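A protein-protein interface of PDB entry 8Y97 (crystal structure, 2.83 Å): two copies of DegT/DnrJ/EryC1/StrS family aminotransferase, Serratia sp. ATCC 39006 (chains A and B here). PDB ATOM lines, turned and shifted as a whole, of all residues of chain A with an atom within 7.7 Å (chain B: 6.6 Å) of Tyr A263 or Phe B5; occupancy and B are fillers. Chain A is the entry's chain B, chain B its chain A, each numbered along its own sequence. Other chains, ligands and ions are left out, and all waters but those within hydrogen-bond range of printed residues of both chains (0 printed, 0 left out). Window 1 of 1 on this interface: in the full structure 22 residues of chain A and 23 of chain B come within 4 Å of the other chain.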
ATOM      1  N   ASN A  42      -7.830   4.975   7.700  1.00  0.00           N
ATOM      2  CA  ASN A  42      -6.795   4.071   7.227  1.00  0.00           C
ATOM      3  C   ASN A  42      -5.585   4.183   8.149  1.00  0.00           C
ATOM      4  O   ASN A  42      -4.692   4.990   7.907  1.00  0.00           O
ATOM      5  CB  ASN A  42      -6.422   4.367   5.778  1.00  0.00           C
ATOM      6  CG  ASN A  42      -7.605   4.272   4.845  1.00  0.00           C
ATOM      7  OD1 ASN A  42      -8.043   3.167   4.514  1.00  0.00           O
ATOM      8  ND2 ASN A  42      -8.122   5.408   4.397  1.00  0.00           N
ATOM      9  N   ALA A  44      -2.224   3.147   9.448  1.00  0.00           N
ATOM     10  CA  ALA A  44      -1.063   2.434   8.946  1.00  0.00           C
ATOM     11  C   ALA A  44       0.086   2.547   9.944  1.00  0.00           C
ATOM     12  O   ALA A  44      -0.023   3.246  10.949  1.00  0.00           O
ATOM     13  CB  ALA A  44      -0.678   2.987   7.594  1.00  0.00           C
ATOM     14  N   LYS A  45       1.184   1.844   9.644  1.00  0.00           N
ATOM     15  CA  LYS A  45       2.390   1.860  10.457  1.00  0.00           C
ATOM     16  C   LYS A  45       2.884   3.292  10.662  1.00  0.00           C
ATOM     17  O   LYS A  45       3.364   3.633  11.740  1.00  0.00           O
ATOM     18  CB  LYS A  45       3.473   1.006   9.788  1.00  0.00           C
ATOM     19  CG  LYS A  45       3.901   1.455   8.394  1.00  0.00           C
ATOM     20  CD  LYS A  45       4.858   0.487   7.713  1.00  0.00           C
ATOM     21  CE  LYS A  45       5.348   1.003   6.400  1.00  0.00           C
ATOM     22  NZ  LYS A  45       6.381   0.129   5.837  1.00  0.00           N
ATOM     23  N   GLU A  46       2.754   4.120   9.617  1.00  0.00           N
ATOM     24  CA  GLU A  46       3.214   5.500   9.644  1.00  0.00           C
ATOM     25  C   GLU A  46       2.575   6.252  10.811  1.00  0.00           C
ATOM     26  O   GLU A  46       3.219   7.089  11.441  1.00  0.00           O
ATOM     27  CB  GLU A  46       2.893   6.213   8.328  1.00  0.00           C
ATOM     28  CG  GLU A  46       3.738   5.756   7.140  1.00  0.00           C
ATOM     29  CD  GLU A  46       3.323   4.467   6.450  1.00  0.00           C
ATOM     30  OE1 GLU A  46       2.236   3.931   6.742  1.00  0.00           O
ATOM     31  OE2 GLU A  46       4.108   3.982   5.611  1.00  0.00           O
ATOM     32  N   GLN A 257      -1.303  11.464   8.565  1.00  0.00           N
ATOM     33  CA  GLN A 257      -2.408  11.250   7.642  1.00  0.00           C
ATOM     34  C   GLN A 257      -2.293  12.166   6.426  1.00  0.00           C
ATOM     35  O   GLN A 257      -2.667  11.773   5.325  1.00  0.00           O
ATOM     36  CB  GLN A 257      -3.753  11.493   8.329  1.00  0.00           C
ATOM     37  CG  GLN A 257      -4.274  10.311   9.139  1.00  0.00           C
ATOM     38  CD  GLN A 257      -4.835   9.200   8.281  1.00  0.00           C
ATOM     39  OE1 GLN A 257      -5.535   9.438   7.288  1.00  0.00           O
ATOM     40  NE2 GLN A 257      -4.525   7.966   8.650  1.00  0.00           N
ATOM     41  N   LEU A 258      -1.788  13.387   6.637  1.00  0.00           N
ATOM     42  CA  LEU A 258      -1.723  14.392   5.587  1.00  0.00           C
ATOM     43  C   LEU A 258      -0.715  13.981   4.513  1.00  0.00           C
ATOM     44  O   LEU A 258      -0.880  14.330   3.346  1.00  0.00           O
ATOM     45  CB  LEU A 258      -1.370  15.743   6.207  1.00  0.00           C
ATOM     46  CG  LEU A 258      -1.492  16.963   5.289  1.00  0.00           C
ATOM     47  CD1 LEU A 258      -2.900  17.104   4.730  1.00  0.00           C
ATOM     48  CD2 LEU A 258      -1.075  18.225   6.036  1.00  0.00           C
ATOM     49  N   ASP A 259       0.318  13.230   4.914  1.00  0.00           N
ATOM     50  CA  ASP A 259       1.333  12.748   3.992  1.00  0.00           C
ATOM     51  C   ASP A 259       0.728  11.784   2.971  1.00  0.00           C
ATOM     52  O   ASP A 259       1.271  11.638   1.877  1.00  0.00           O
ATOM     53  CB  ASP A 259       2.484  12.084   4.735  1.00  0.00           C
ATOM     54  CG  ASP A 259       3.388  13.006   5.539  1.00  0.00           C
ATOM     55  OD1 ASP A 259       3.338  14.234   5.298  1.00  0.00           O
ATOM     56  OD2 ASP A 259       4.118  12.482   6.413  1.00  0.00           O
ATOM     57  N   ARG A 260      -0.385  11.128   3.330  1.00  0.00           N
ATOM     58  CA  ARG A 260      -0.961  10.083   2.499  1.00  0.00           C
ATOM     59  C   ARG A 260      -2.367  10.456   2.032  1.00  0.00           C
ATOM     60  O   ARG A 260      -3.072   9.601   1.506  1.00  0.00           O
ATOM     61  CB  ARG A 260      -1.029   8.762   3.274  1.00  0.00           C
ATOM     62  CG  ARG A 260       0.212   8.444   4.094  1.00  0.00           C
ATOM     63  CD  ARG A 260       0.304   6.966   4.447  1.00  0.00           C
ATOM     64  NE  ARG A 260      -0.886   6.434   5.121  1.00  0.00           N
ATOM     65  CZ  ARG A 260      -1.241   6.688   6.377  1.00  0.00           C
ATOM     66  NH1 ARG A 260      -0.531   7.518   7.122  1.00  0.00           N
ATOM     67  NH2 ARG A 260      -2.317   6.113   6.888  1.00  0.00           N
ATOM     68  N   LEU A 261      -2.765  11.726   2.196  1.00  0.00           N
ATOM     69  CA  LEU A 261      -4.132  12.136   1.908  1.00  0.00           C
ATOM     70  C   LEU A 261      -4.399  12.049   0.406  1.00  0.00           C
ATOM     71  O   LEU A 261      -5.423  11.503  -0.002  1.00  0.00           O
ATOM     72  CB  LEU A 261      -4.409  13.541   2.444  1.00  0.00           C
ATOM     73  CG  LEU A 261      -5.803  14.116   2.162  1.00  0.00           C
ATOM     74  CD1 LEU A 261      -6.911  13.218   2.684  1.00  0.00           C
ATOM     75  CD2 LEU A 261      -5.934  15.505   2.758  1.00  0.00           C
ATOM     76  N   ASP A 262      -3.475  12.587  -0.402  1.00  0.00           N
ATOM     77  CA  ASP A 262      -3.644  12.666  -1.846  1.00  0.00           C
ATOM     78  C   ASP A 262      -3.854  11.273  -2.436  1.00  0.00           C
ATOM     79  O   ASP A 262      -4.647  11.110  -3.359  1.00  0.00           O
ATOM     80  CB  ASP A 262      -2.470  13.374  -2.507  1.00  0.00           C
ATOM     81  CG  ASP A 262      -2.437  14.890  -2.367  1.00  0.00           C
ATOM     82  OD1 ASP A 262      -3.461  15.470  -1.948  1.00  0.00           O
ATOM     83  OD2 ASP A 262      -1.383  15.480  -2.677  1.00  0.00           O
ATOM     84  N   TYR A 263      -3.134  10.279  -1.900  1.00  0.00           N
ATOM     85  CA  TYR A 263      -3.269   8.905  -2.352  1.00  0.00           C
ATOM     86  C   TYR A 263      -4.713   8.449  -2.166  1.00  0.00           C
ATOM     87  O   TYR A 263      -5.347   7.998  -3.115  1.00  0.00           O
ATOM     88  CB  TYR A 263      -2.290   7.986  -1.611  1.00  0.00           C
ATOM     89  CG  TYR A 263      -2.526   6.501  -1.854  1.00  0.00           C
ATOM     90  CD1 TYR A 263      -2.146   5.899  -3.049  1.00  0.00           C
ATOM     91  CD2 TYR A 263      -3.131   5.701  -0.890  1.00  0.00           C
ATOM     92  CE1 TYR A 263      -2.362   4.549  -3.279  1.00  0.00           C
ATOM     93  CE2 TYR A 263      -3.350   4.350  -1.106  1.00  0.00           C
ATOM     94  CZ  TYR A 263      -2.962   3.773  -2.303  1.00  0.00           C
ATOM     95  OH  TYR A 263      -3.175   2.443  -2.522  1.00  0.00           O
ATOM     96  N   TYR A 264      -5.222   8.581  -0.935  1.00  0.00           N
ATOM     97  CA  TYR A 264      -6.559   8.120  -0.594  1.00  0.00           C
ATOM     98  C   TYR A 264      -7.602   8.891  -1.405  1.00  0.00           C
ATOM     99  O   TYR A 264      -8.559   8.295  -1.889  1.00  0.00           O
ATOM    100  CB  TYR A 264      -6.792   8.259   0.915  1.00  0.00           C
ATOM    101  CG  TYR A 264      -5.902   7.399   1.803  1.00  0.00           C
ATOM    102  CD1 TYR A 264      -5.685   6.056   1.524  1.00  0.00           C
ATOM    103  CD2 TYR A 264      -5.280   7.935   2.926  1.00  0.00           C
ATOM    104  CE1 TYR A 264      -4.874   5.273   2.329  1.00  0.00           C
ATOM    105  CE2 TYR A 264      -4.465   7.164   3.739  1.00  0.00           C
ATOM    106  CZ  TYR A 264      -4.262   5.828   3.440  1.00  0.00           C
ATOM    107  OH  TYR A 264      -3.462   5.056   4.233  1.00  0.00           O
ATOM    108  N   ASP A 265      -7.402  10.208  -1.557  1.00  0.00           N
ATOM    109  CA  ASP A 265      -8.326  11.066  -2.285  1.00  0.00           C
ATOM    110  C   ASP A 265      -8.482  10.598  -3.728  1.00  0.00           C
ATOM    111  O   ASP A 265      -9.578  10.667  -4.274  1.00  0.00           O
ATOM    112  CB  ASP A 265      -7.876  12.520  -2.294  1.00  0.00           C
ATOM    113  CG  ASP A 265      -8.095  13.301  -1.008  1.00  0.00           C
ATOM    114  OD1 ASP A 265      -8.656  12.728  -0.055  1.00  0.00           O
ATOM    115  OD2 ASP A 265      -7.702  14.483  -0.975  1.00  0.00           O
ATOM    116  N   GLU A 266      -7.376  10.151  -4.338  1.00  0.00           N
ATOM    117  CA  GLU A 266      -7.363   9.747  -5.735  1.00  0.00           C
ATOM    118  C   GLU A 266      -8.246   8.515  -5.924  1.00  0.00           C
ATOM    119  O   GLU A 266      -9.049   8.477  -6.851  1.00  0.00           O
ATOM    120  CB  GLU A 266      -5.931   9.489  -6.209  1.00  0.00           C
ATOM    121  CG  GLU A 266      -5.809   9.181  -7.702  1.00  0.00           C
ATOM    122  CD  GLU A 266      -6.266  10.292  -8.635  1.00  0.00           C
ATOM    123  OE1 GLU A 266      -6.007  11.466  -8.301  1.00  0.00           O
ATOM    124  OE2 GLU A 266      -6.842   9.988  -9.705  1.00  0.00           O
ATOM    125  N   ILE A 267      -8.096   7.518  -5.040  1.00  0.00           N
ATOM    126  CA  ILE A 267      -8.938   6.330  -5.075  1.00  0.00           C
ATOM    127  C   ILE A 267     -10.393   6.752  -4.880  1.00  0.00           C
ATOM    128  O   ILE A 267     -11.285   6.246  -5.561  1.00  0.00           O
ATOM    129  CB  ILE A 267      -8.498   5.295  -4.021  1.00  0.00           C
ATOM    130  CG1 ILE A 267      -7.080   4.780  -4.295  1.00  0.00           C
ATOM    131  CG2 ILE A 267      -9.505   4.146  -3.936  1.00  0.00           C
ATOM    132  CD1 ILE A 267      -6.501   3.920  -3.187  1.00  0.00           C
ATOM    133  N   ARG A 268     -10.609   7.691  -3.953  1.00  0.00           N
ATOM    134  CA  ARG A 268     -11.937   8.163  -3.594  1.00  0.00           C
ATOM    135  C   ARG A 268     -12.608   8.795  -4.813  1.00  0.00           C
ATOM    136  O   ARG A 268     -13.777   8.529  -5.079  1.00  0.00           O
ATOM    137  CB  ARG A 268     -11.809   9.146  -2.423  1.00  0.00           C
ATOM    138  CG  ARG A 268     -12.805   8.926  -1.291  1.00  0.00           C
ATOM    139  CD  ARG A 268     -12.516   9.823  -0.087  1.00  0.00           C
ATOM    140  NE  ARG A 268     -11.557   9.221   0.849  1.00  0.00           N
ATOM    141  CZ  ARG A 268     -10.455   9.786   1.345  1.00  0.00           C
ATOM    142  NH1 ARG A 268     -10.075  10.988   0.953  1.00  0.00           N
ATOM    143  NH2 ARG A 268      -9.725   9.137   2.240  1.00  0.00           N
ATOM    144  N   GLN A 269     -11.852   9.618  -5.553  1.00  0.00           N
ATOM    145  CA  GLN A 269     -12.352  10.312  -6.732  1.00  0.00           C
ATOM    146  C   GLN A 269     -12.713   9.324  -7.839  1.00  0.00           C
ATOM    147  O   GLN A 269     -13.800   9.409  -8.406  1.00  0.00           O
ATOM    148  CB  GLN A 269     -11.339  11.317  -7.286  1.00  0.00           C
ATOM    149  CG  GLN A 269     -11.589  12.753  -6.839  1.00  0.00           C
ATOM    150  CD  GLN A 269     -12.836  13.352  -7.453  1.00  0.00           C
ATOM    151  OE1 GLN A 269     -13.260  12.981  -8.551  1.00  0.00           O
ATOM    152  NE2 GLN A 269     -13.436  14.299  -6.751  1.00  0.00           N
ATOM    153  N   ARG A 270     -11.787   8.411  -8.156  1.00  0.00           N
ATOM    154  CA  ARG A 270     -11.957   7.490  -9.269  1.00  0.00           C
ATOM    155  C   ARG A 270     -13.102   6.523  -8.983  1.00  0.00           C
ATOM    156  O   ARG A 270     -13.842   6.163  -9.893  1.00  0.00           O
ATOM    157  CB  ARG A 270     -10.669   6.713  -9.566  1.00  0.00           C
ATOM    158  CG  ARG A 270      -9.530   7.589 -10.069  1.00  0.00           C
ATOM    159  CD  ARG A 270      -8.427   6.774 -10.734  1.00  0.00           C
ATOM    160  NE  ARG A 270      -7.148   7.477 -10.894  1.00  0.00           N
ATOM    161  CZ  ARG A 270      -5.936   6.965 -10.654  1.00  0.00           C
ATOM    162  NH1 ARG A 270      -5.799   5.768 -10.105  1.00  0.00           N
ATOM    163  NH2 ARG A 270      -4.860   7.670 -10.955  1.00  0.00           N
ATOM    164  N   PRO A 394     -11.440   4.398   0.872  1.00  0.00           N
ATOM    165  CA  PRO A 394     -10.949   4.168  -0.488  1.00  0.00           C
ATOM    166  C   PRO A 394     -10.941   2.674  -0.796  1.00  0.00           C
ATOM    167  O   PRO A 394      -9.900   2.024  -0.710  1.00  0.00           O
ATOM    168  CB  PRO A 394      -9.547   4.791  -0.448  1.00  0.00           C
ATOM    169  CG  PRO A 394      -9.096   4.561   0.980  1.00  0.00           C
ATOM    170  CD  PRO A 394     -10.357   4.695   1.823  1.00  0.00           C
ATOM    171  N   THR B   3       9.575   6.435   4.569  1.00  0.00           N
ATOM    172  CA  THR B   3       8.531   5.438   4.401  1.00  0.00           C
ATOM    173  C   THR B   3       8.559   4.914   2.967  1.00  0.00           C
ATOM    174  O   THR B   3       8.936   5.633   2.044  1.00  0.00           O
ATOM    175  CB  THR B   3       7.173   6.046   4.758  1.00  0.00           C
ATOM    176  OG1 THR B   3       6.214   5.027   4.497  1.00  0.00           O
ATOM    177  CG2 THR B   3       6.828   7.277   3.939  1.00  0.00           C
ATOM    178  N   ASP B   4       8.125   3.660   2.799  1.00  0.00           N
ATOM    179  CA  ASP B   4       8.064   3.017   1.496  1.00  0.00           C
ATOM    180  C   ASP B   4       6.700   3.254   0.847  1.00  0.00           C
ATOM    181  O   ASP B   4       6.453   2.778  -0.257  1.00  0.00           O
ATOM    182  CB  ASP B   4       8.366   1.529   1.607  1.00  0.00           C
ATOM    183  CG  ASP B   4       7.485   0.741   2.568  1.00  0.00           C
ATOM    184  OD1 ASP B   4       6.730   1.376   3.333  1.00  0.00           O
ATOM    185  OD2 ASP B   4       7.546  -0.504   2.539  1.00  0.00           O
ATOM    186  N   PHE B   5       5.820   3.995   1.528  1.00  0.00           N
ATOM    187  CA  PHE B   5       4.430   4.105   1.116  1.00  0.00           C
ATOM    188  C   PHE B   5       4.353   4.673  -0.299  1.00  0.00           C
ATOM    189  O   PHE B   5       4.951   5.707  -0.591  1.00  0.00           O
ATOM    190  CB  PHE B   5       3.660   4.962   2.125  1.00  0.00           C
ATOM    191  CG  PHE B   5       2.162   5.013   1.867  1.00  0.00           C
ATOM    192  CD1 PHE B   5       1.319   4.027   2.371  1.00  0.00           C
ATOM    193  CD2 PHE B   5       1.603   6.036   1.105  1.00  0.00           C
ATOM    194  CE1 PHE B   5      -0.045   4.068   2.126  1.00  0.00           C
ATOM    195  CE2 PHE B   5       0.237   6.074   0.866  1.00  0.00           C
ATOM    196  CZ  PHE B   5      -0.583   5.093   1.380  1.00  0.00           C
ATOM    197  N   ILE B   6       3.601   3.980  -1.163  1.00  0.00           N
ATOM    198  CA  ILE B   6       3.405   4.383  -2.546  1.00  0.00           C
ATOM    199  C   ILE B   6       2.284   5.417  -2.591  1.00  0.00           C
ATOM    200  O   ILE B   6       1.194   5.165  -2.084  1.00  0.00           O
ATOM    201  CB  ILE B   6       3.088   3.156  -3.423  1.00  0.00           C
ATOM    202  CG1 ILE B   6       4.201   2.111  -3.364  1.00  0.00           C
ATOM    203  CG2 ILE B   6       2.794   3.569  -4.863  1.00  0.00           C
ATOM    204  CD1 ILE B   6       3.769   0.720  -3.794  1.00  0.00           C
ATOM    205  N   MET B   7       2.558   6.564  -3.226  1.00  0.00           N
ATOM    206  CA  MET B   7       1.664   7.711  -3.194  1.00  0.00           C
ATOM    207  C   MET B   7       0.755   7.760  -4.423  1.00  0.00           C
ATOM    208  O   MET B   7      -0.247   8.469  -4.413  1.00  0.00           O
ATOM    209  CB  MET B   7       2.460   9.018  -3.115  1.00  0.00           C
ATOM    210  CG  MET B   7       3.069   9.294  -1.752  1.00  0.00           C
ATOM    211  SD  MET B   7       1.840   9.423  -0.436  1.00  0.00           S
ATOM    212  CE  MET B   7       0.735  10.709  -1.041  1.00  0.00           C
ATOM    213  N   VAL B   8       1.109   7.024  -5.483  1.00  0.00           N
ATOM    214  CA  VAL B   8       0.334   7.028  -6.714  1.00  0.00           C
ATOM    215  C   VAL B   8      -0.403   5.696  -6.816  1.00  0.00           C
ATOM    216  O   VAL B   8       0.233   4.645  -6.825  1.00  0.00           O
ATOM    217  CB  VAL B   8       1.215   7.269  -7.956  1.00  0.00           C
ATOM    218  CG1 VAL B   8       0.377   7.474  -9.211  1.00  0.00           C
ATOM    219  CG2 VAL B   8       2.163   8.446  -7.764  1.00  0.00           C
ATOM    220  N   PRO B   9      -1.756   5.690  -6.896  1.00  0.00           N
ATOM    221  CA  PRO B   9      -2.512   4.452  -7.083  1.00  0.00           C
ATOM    222  C   PRO B   9      -2.380   3.964  -8.521  1.00  0.00           C
ATOM    223  O   PRO B   9      -2.251   4.768  -9.442  1.00  0.00           O
ATOM    224  CB  PRO B   9      -3.971   4.801  -6.730  1.00  0.00           C
ATOM    225  CG  PRO B   9      -3.961   6.270  -6.349  1.00  0.00           C
ATOM    226  CD  PRO B   9      -2.635   6.864  -6.807  1.00  0.00           C
ATOM    227  N   THR B  10      -2.422   2.637  -8.699  1.00  0.00           N
ATOM    228  CA  THR B  10      -2.347   2.040 -10.021  1.00  0.00           C
ATOM    229  C   THR B  10      -3.699   2.223 -10.705  1.00  0.00           C
ATOM    230  O   THR B  10      -4.691   1.630 -10.288  1.00  0.00           O
ATOM    231  CB  THR B  10      -1.963   0.565  -9.914  1.00  0.00           C
ATOM    232  OG1 THR B  10      -0.790   0.521  -9.107  1.00  0.00           O
ATOM    233  CG2 THR B  10      -1.674  -0.053 -11.270  1.00  0.00           C
ATOM    234  N   LYS B  37       6.562  -0.003  -8.473  1.00  0.00           N
ATOM    235  CA  LYS B  37       7.027  -0.453  -7.170  1.00  0.00           C
ATOM    236  C   LYS B  37       5.950  -1.332  -6.536  1.00  0.00           C
ATOM    237  O   LYS B  37       4.763  -1.140  -6.785  1.00  0.00           O
ATOM    238  CB  LYS B  37       7.369   0.731  -6.257  1.00  0.00           C
ATOM    239  CG  LYS B  37       8.121   1.881  -6.920  1.00  0.00           C
ATOM    240  CD  LYS B  37       7.229   2.993  -7.465  1.00  0.00           C
ATOM    241  CE  LYS B  37       6.769   3.950  -6.409  1.00  0.00           C
ATOM    242  NZ  LYS B  37       7.854   4.838  -5.976  1.00  0.00           N
ATOM    243  N   ILE B  39       5.165  -3.294  -2.492  1.00  0.00           N
ATOM    244  CA  ILE B  39       5.544  -3.367  -1.092  1.00  0.00           C
ATOM    245  C   ILE B  39       5.593  -4.836  -0.690  1.00  0.00           C
ATOM    246  O   ILE B  39       4.618  -5.564  -0.868  1.00  0.00           O
ATOM    247  CB  ILE B  39       4.557  -2.578  -0.209  1.00  0.00           C
ATOM    248  CG1 ILE B  39       4.432  -1.113  -0.643  1.00  0.00           C
ATOM    249  CG2 ILE B  39       4.929  -2.704   1.269  1.00  0.00           C
ATOM    250  CD1 ILE B  39       5.740  -0.344  -0.619  1.00  0.00           C
ATOM    251  N   GLU B 396      -3.208  -5.460  -5.963  1.00  0.00           N
ATOM    252  CA  GLU B 396      -4.594  -5.086  -6.198  1.00  0.00           C
ATOM    253  C   GLU B 396      -4.994  -5.481  -7.619  1.00  0.00           C
ATOM    254  O   GLU B 396      -4.137  -5.806  -8.438  1.00  0.00           O
ATOM    255  CB  GLU B 396      -4.821  -3.596  -5.913  1.00  0.00           C
ATOM    256  CG  GLU B 396      -4.127  -2.623  -6.868  1.00  0.00           C
ATOM    257  CD  GLU B 396      -2.653  -2.332  -6.626  1.00  0.00           C
ATOM    258  OE1 GLU B 396      -2.003  -3.051  -5.834  1.00  0.00           O
ATOM    259  OE2 GLU B 396      -2.153  -1.360  -7.236  1.00  0.00           O
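Of chain B, only Phe B5, Ile B6, Met B7 and Pro B9 come within 4 Å of Tyr A263. Printed residues of chain B within 4 Å of Glu A266: Pro B9. Printed residues of chain B within 4 Å of Glu A46: Thr B3 (2.6 Å) and Phe B5 (3.6 Å). Printed residues of chain B within 4 Å of Lys A45: Asp B4. Ile B39 touches none of the printed residues of chain A. Gln A269 touches none of the printed residues of chain B. The nearest residue of chain B that does not touch Tyr A263 is Val B8 (4.2 Å). The nearest printed residue of chain A that does not touch Pro B9 is Asp A262 (5.7 Å).
Phe B5 touches Glu A46. CD of Arg A260 touches CE2 of Phe B5 (3.7 Å). Met B7 touches Arg A260 (CE to CA, 3.97 Å). Tyr A263 touches Phe B5 (CD2 to CZ, 3.5 Å). Tyr A263 touches Ile B6. Tyr A263 touches Met B7 (CD1 to O, 3.5 Å). Pro B9 touches Tyr A263. Glu A266 touches Pro B9 (CG to CG, 3.7 Å). CB of Pro B9 touches CG1 of Ile A267, at 3.9 Å. Pro B9 touches Arg A270 (O to NH1, 3.7 Å).
Of the 11 printed residues of chain B, 6 touch a printed residue of chain A. Of the 19 printed residues of chain A, 8 touch a printed residue of chain B.
The side-chain amide nitrogen of Gln A257 sits close to the guanidinium group of Arg A260, at 3.4 Å. The side-chain hydroxyl of Thr B3 sits at hydrogen-bond distance from the backbone NH of Phe B5, at 3.2 Å. OH of Tyr A264 is in hydrogen-bond range of NE of Arg A260 (3.1 Å). The backbone carbonyl oxygen (O) of Asn A42 sits at hydrogen-bond distance from the guanidinium group (NH2) of Arg A260 (2.8 Å). OE2 of Glu A266 is in salt-bridge range of NE of Arg A270, at 2.8 Å.
No position is printed for both chains. Of the 13 pairs that touch across the chains among the printed residues, none has its exchanged pair printed and touching as well.
The side-chain carboxylate of Asp B4 lies within salt-bridge range of the side-chain amino group of Lys A45, at 2.8 Å. The side-chain carboxylate of Glu A46 is in hydrogen-bond range of the side-chain hydroxyl of Thr B3 (2.6 Å). The backbone carbonyl oxygen (O) of Asp A259 lies close to the side-chain sulfur (SD) of Met B7 (3.3 Å).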
